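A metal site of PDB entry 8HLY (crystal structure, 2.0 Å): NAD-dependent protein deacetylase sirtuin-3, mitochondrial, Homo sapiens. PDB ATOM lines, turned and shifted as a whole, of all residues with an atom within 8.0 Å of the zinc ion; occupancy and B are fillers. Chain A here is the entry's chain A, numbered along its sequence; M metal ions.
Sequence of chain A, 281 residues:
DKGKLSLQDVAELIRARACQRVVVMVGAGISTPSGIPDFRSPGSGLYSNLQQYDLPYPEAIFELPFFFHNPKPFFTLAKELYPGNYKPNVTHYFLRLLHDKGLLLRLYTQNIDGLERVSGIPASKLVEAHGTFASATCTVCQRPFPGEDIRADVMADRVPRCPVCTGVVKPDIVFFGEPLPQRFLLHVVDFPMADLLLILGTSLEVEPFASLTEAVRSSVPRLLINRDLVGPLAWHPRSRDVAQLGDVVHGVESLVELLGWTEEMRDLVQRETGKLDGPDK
The guanidinium group (NH1) of Arg 143 lies close to the side-chain sulfur (SG) of Cys 141 (3.2 Å).
The backbone NH (N) of Gly 167 lies close to the side-chain sulfur (SG) of Cys 165, 3.5 Å away.
SG of Cys 138 lies close to N of Val 140.
The backbone NH (N) of Cys 138 lies within hydrogen-bond range of the backbone carbonyl oxygen (O) of Arg 143 (2.9 Å).
The backbone NH (N) of Cys 162 sits at hydrogen-bond distance from the backbone carbonyl oxygen (O) of Gly 167.
The backbone NH of Val 164 lies close to the side-chain sulfur of Cys 162, at 3.4 Å.
Of the 18 residues printed, 4 come within 4 Å of the zinc ion.
The zinc ion is bound by the side-chain sulfur (SG) of Cys 141, 2.3 Å away.
The zinc ion is bound by SG of Cys 165 (2.3 Å).
The side-chain sulfur (SG) of Cys 138 is bound to the zinc ion (2.3 Å).
The zinc ion is bound by the side-chain sulfur (SG) of Cys 162, at 2.4 Å.
The zinc ion has four donor atoms within binding distance.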
ATOM      1  N   THR A 137      27.530  -7.431  -8.259  1.00  0.00           N
ATOM      2  CA  THR A 137      26.682  -7.444  -9.446  1.00  0.00           C
ATOM      3  C   THR A 137      25.220  -7.380  -9.019  1.00  0.00           C
ATOM      4  O   THR A 137      24.789  -8.147  -8.167  1.00  0.00           O
ATOM      5  CB  THR A 137      26.919  -8.714 -10.272  1.00  0.00           C
ATOM      6  OG1 THR A 137      28.285  -8.769 -10.694  1.00  0.00           O
ATOM      7  CG2 THR A 137      26.005  -8.750 -11.511  1.00  0.00           C
ATOM      8  N   CYS A 138      24.459  -6.455  -9.620  1.00  0.00           N
ATOM      9  CA  CYS A 138      23.017  -6.441  -9.387  1.00  0.00           C
ATOM     10  C   CYS A 138      22.395  -7.750  -9.849  1.00  0.00           C
ATOM     11  O   CYS A 138      22.615  -8.183 -10.990  1.00  0.00           O
ATOM     12  CB  CYS A 138      22.368  -5.274 -10.109  1.00  0.00           C
ATOM     13  SG  CYS A 138      20.574  -5.238  -9.901  1.00  0.00           S
ATOM     14  N   THR A 139      21.618  -8.393  -8.974  1.00  0.00           N
ATOM     15  CA  THR A 139      21.013  -9.679  -9.304  1.00  0.00           C
ATOM     16  C   THR A 139      19.844  -9.545 -10.277  1.00  0.00           C
ATOM     17  O   THR A 139      19.401 -10.559 -10.818  1.00  0.00           O
ATOM     18  CB  THR A 139      20.534 -10.415  -8.048  1.00  0.00           C
ATOM     19  OG1 THR A 139      19.506  -9.647  -7.397  1.00  0.00           O
ATOM     20  CG2 THR A 139      21.696 -10.649  -7.087  1.00  0.00           C
ATOM     21  N   VAL A 140      19.337  -8.337 -10.482  1.00  0.00           N
ATOM     22  CA  VAL A 140      18.198  -8.097 -11.362  1.00  0.00           C
ATOM     23  C   VAL A 140      18.642  -7.632 -12.745  1.00  0.00           C
ATOM     24  O   VAL A 140      18.304  -8.246 -13.745  1.00  0.00           O
ATOM     25  CB  VAL A 140      17.221  -7.100 -10.702  1.00  0.00           C
ATOM     26  CG1 VAL A 140      16.107  -6.702 -11.656  1.00  0.00           C
ATOM     27  CG2 VAL A 140      16.639  -7.712  -9.436  1.00  0.00           C
ATOM     28  N   CYS A 141      19.448  -6.558 -12.810  1.00  0.00           N
ATOM     29  CA  CYS A 141      19.837  -5.971 -14.085  1.00  0.00           C
ATOM     30  C   CYS A 141      21.263  -6.314 -14.513  1.00  0.00           C
ATOM     31  O   CYS A 141      21.629  -6.030 -15.658  1.00  0.00           O
ATOM     32  CB  CYS A 141      19.682  -4.436 -14.037  1.00  0.00           C
ATOM     33  SG  CYS A 141      20.991  -3.548 -13.168  1.00  0.00           S
ATOM     34  N   GLN A 142      22.058  -6.931 -13.639  1.00  0.00           N
ATOM     35  CA  GLN A 142      23.419  -7.385 -13.898  1.00  0.00           C
ATOM     36  C   GLN A 142      24.430  -6.255 -14.005  1.00  0.00           C
ATOM     37  O   GLN A 142      25.562  -6.492 -14.446  1.00  0.00           O
ATOM     38  CB  GLN A 142      23.499  -8.254 -15.151  1.00  0.00           C
ATOM     39  CG  GLN A 142      22.616  -9.502 -15.122  1.00  0.00           C
ATOM     40  CD  GLN A 142      22.953 -10.454 -13.974  1.00  0.00           C
ATOM     41  OE1 GLN A 142      24.119 -10.757 -13.731  1.00  0.00           O
ATOM     42  NE2 GLN A 142      21.926 -10.922 -13.279  1.00  0.00           N
ATOM     43  N   ARG A 143      24.095  -5.039 -13.603  1.00  0.00           N
ATOM     44  CA  ARG A 143      25.096  -3.981 -13.598  1.00  0.00           C
ATOM     45  C   ARG A 143      26.177  -4.292 -12.554  1.00  0.00           C
ATOM     46  O   ARG A 143      25.862  -4.769 -11.458  1.00  0.00           O
ATOM     47  CB  ARG A 143      24.458  -2.621 -13.298  1.00  0.00           C
ATOM     48  CG  ARG A 143      23.899  -1.932 -14.528  1.00  0.00           C
ATOM     49  CD  ARG A 143      23.154  -0.657 -14.160  1.00  0.00           C
ATOM     50  NE  ARG A 143      22.613   0.013 -15.342  1.00  0.00           N
ATOM     51  CZ  ARG A 143      21.520  -0.363 -15.981  1.00  0.00           C
ATOM     52  NH1 ARG A 143      20.826  -1.420 -15.603  1.00  0.00           N
ATOM     53  NH2 ARG A 143      21.106   0.339 -17.032  1.00  0.00           N
ATOM     54  N   PRO A 144      27.452  -4.057 -12.872  1.00  0.00           N
ATOM     55  CA  PRO A 144      28.514  -4.286 -11.888  1.00  0.00           C
ATOM     56  C   PRO A 144      28.779  -3.051 -11.049  1.00  0.00           C
ATOM     57  O   PRO A 144      28.505  -1.916 -11.449  1.00  0.00           O
ATOM     58  CB  PRO A 144      29.730  -4.621 -12.774  1.00  0.00           C
ATOM     59  CG  PRO A 144      29.497  -3.760 -14.003  1.00  0.00           C
ATOM     60  CD  PRO A 144      27.984  -3.660 -14.186  1.00  0.00           C
ATOM     61  N   PHE A 145      29.345  -3.284  -9.855  1.00  0.00           N
ATOM     62  CA  PHE A 145      29.670  -2.208  -8.930  1.00  0.00           C
ATOM     63  C   PHE A 145      30.972  -2.525  -8.194  1.00  0.00           C
ATOM     64  O   PHE A 145      31.223  -3.703  -7.873  1.00  0.00           O
ATOM     65  CB  PHE A 145      28.562  -1.980  -7.897  1.00  0.00           C
ATOM     66  CG  PHE A 145      27.246  -1.612  -8.494  1.00  0.00           C
ATOM     67  CD1 PHE A 145      26.952  -0.287  -8.764  1.00  0.00           C
ATOM     68  CD2 PHE A 145      26.303  -2.575  -8.791  1.00  0.00           C
ATOM     69  CE1 PHE A 145      25.746   0.070  -9.332  1.00  0.00           C
ATOM     70  CE2 PHE A 145      25.097  -2.219  -9.359  1.00  0.00           C
ATOM     71  CZ  PHE A 145      24.818  -0.910  -9.625  1.00  0.00           C
ATOM     72  N   ARG A 161      21.285  -2.140  -2.537  1.00  0.00           N
ATOM     73  CA  ARG A 161      20.376  -2.202  -3.671  1.00  0.00           C
ATOM     74  C   ARG A 161      20.881  -1.346  -4.819  1.00  0.00           C
ATOM     75  O   ARG A 161      21.629  -0.379  -4.621  1.00  0.00           O
ATOM     76  CB  ARG A 161      18.956  -1.784  -3.252  1.00  0.00           C
ATOM     77  CG  ARG A 161      18.260  -2.848  -2.384  1.00  0.00           C
ATOM     78  CD  ARG A 161      16.800  -2.561  -2.134  1.00  0.00           C
ATOM     79  NE  ARG A 161      16.144  -3.648  -1.424  1.00  0.00           N
ATOM     80  CZ  ARG A 161      15.598  -4.704  -2.012  1.00  0.00           C
ATOM     81  NH1 ARG A 161      15.566  -4.834  -3.322  1.00  0.00           N
ATOM     82  NH2 ARG A 161      15.061  -5.668  -1.252  1.00  0.00           N
ATOM     83  N   CYS A 162      20.487  -1.723  -6.023  1.00  0.00           N
ATOM     84  CA  CYS A 162      21.023  -1.115  -7.246  1.00  0.00           C
ATOM     85  C   CYS A 162      20.447   0.288  -7.449  1.00  0.00           C
ATOM     86  O   CYS A 162      19.238   0.481  -7.315  1.00  0.00           O
ATOM     87  CB  CYS A 162      20.658  -2.022  -8.433  1.00  0.00           C
ATOM     88  SG  CYS A 162      20.995  -1.368 -10.076  1.00  0.00           S
ATOM     89  N   PRO A 163      21.278   1.290  -7.781  1.00  0.00           N
ATOM     90  CA  PRO A 163      20.740   2.641  -7.983  1.00  0.00           C
ATOM     91  C   PRO A 163      19.878   2.774  -9.230  1.00  0.00           C
ATOM     92  O   PRO A 163      19.156   3.774  -9.346  1.00  0.00           O
ATOM     93  CB  PRO A 163      21.994   3.528  -8.109  1.00  0.00           C
ATOM     94  CG  PRO A 163      23.094   2.721  -7.551  1.00  0.00           C
ATOM     95  CD  PRO A 163      22.753   1.286  -7.825  1.00  0.00           C
ATOM     96  N   VAL A 164      19.925   1.815 -10.147  1.00  0.00           N
ATOM     97  CA  VAL A 164      19.108   1.888 -11.358  1.00  0.00           C
ATOM     98  C   VAL A 164      17.783   1.171 -11.181  1.00  0.00           C
ATOM     99  O   VAL A 164      16.714   1.752 -11.403  1.00  0.00           O
ATOM    100  CB  VAL A 164      19.896   1.329 -12.564  1.00  0.00           C
ATOM    101  CG1 VAL A 164      18.997   1.339 -13.811  1.00  0.00           C
ATOM    102  CG2 VAL A 164      21.165   2.126 -12.798  1.00  0.00           C
ATOM    103  N   CYS A 165      17.810  -0.105 -10.786  1.00  0.00           N
ATOM    104  CA  CYS A 165      16.593  -0.905 -10.737  1.00  0.00           C
ATOM    105  C   CYS A 165      16.161  -1.303  -9.327  1.00  0.00           C
ATOM    106  O   CYS A 165      15.076  -1.870  -9.182  1.00  0.00           O
ATOM    107  CB  CYS A 165      16.773  -2.168 -11.600  1.00  0.00           C
ATOM    108  SG  CYS A 165      17.732  -3.485 -10.836  1.00  0.00           S
ATOM    109  N   THR A 166      16.953  -0.987  -8.307  1.00  0.00           N
ATOM    110  CA  THR A 166      16.688  -1.257  -6.890  1.00  0.00           C
ATOM    111  C   THR A 166      16.782  -2.736  -6.518  1.00  0.00           C
ATOM    112  O   THR A 166      16.444  -3.096  -5.382  1.00  0.00           O
ATOM    113  CB  THR A 166      15.316  -0.740  -6.419  1.00  0.00           C
ATOM    114  OG1 THR A 166      14.281  -1.635  -6.828  1.00  0.00           O
ATOM    115  CG2 THR A 166      15.024   0.651  -6.947  1.00  0.00           C
ATOM    116  N   GLY A 167      17.242  -3.594  -7.417  1.00  0.00           N
ATOM    117  CA  GLY A 167      17.466  -4.979  -7.062  1.00  0.00           C
ATOM    118  C   GLY A 167      18.631  -5.142  -6.092  1.00  0.00           C
ATOM    119  O   GLY A 167      19.481  -4.262  -5.938  1.00  0.00           O
ATOM    120  N   VAL A 168      18.671  -6.299  -5.445  1.00  0.00           N
ATOM    121  CA  VAL A 168      19.730  -6.564  -4.473  1.00  0.00           C
ATOM    122  C   VAL A 168      21.049  -6.773  -5.207  1.00  0.00           C
ATOM    123  O   VAL A 168      21.134  -7.533  -6.176  1.00  0.00           O
ATOM    124  CB  VAL A 168      19.390  -7.768  -3.601  1.00  0.00           C
ATOM    125  CG1 VAL A 168      20.609  -8.190  -2.771  1.00  0.00           C
ATOM    126  CG2 VAL A 168      18.229  -7.430  -2.702  1.00  0.00           C
ATOM    127  N   VAL A 169      22.093  -6.099  -4.729  1.00  0.00           N
ATOM    128  CA  VAL A 169      23.418  -6.174  -5.307  1.00  0.00           C
ATOM    129  C   VAL A 169      24.200  -7.217  -4.531  1.00  0.00           C
ATOM    130  O   VAL A 169      24.356  -7.101  -3.308  1.00  0.00           O
ATOM    131  CB  VAL A 169      24.113  -4.805  -5.277  1.00  0.00           C
ATOM    132  CG1 VAL A 169      25.547  -4.906  -5.789  1.00  0.00           C
ATOM    133  CG2 VAL A 169      23.304  -3.795  -6.087  1.00  0.00           C
HETATM  134 ZN    ZN M   1      20.043  -3.280 -11.061  1.00  0.00          ZN
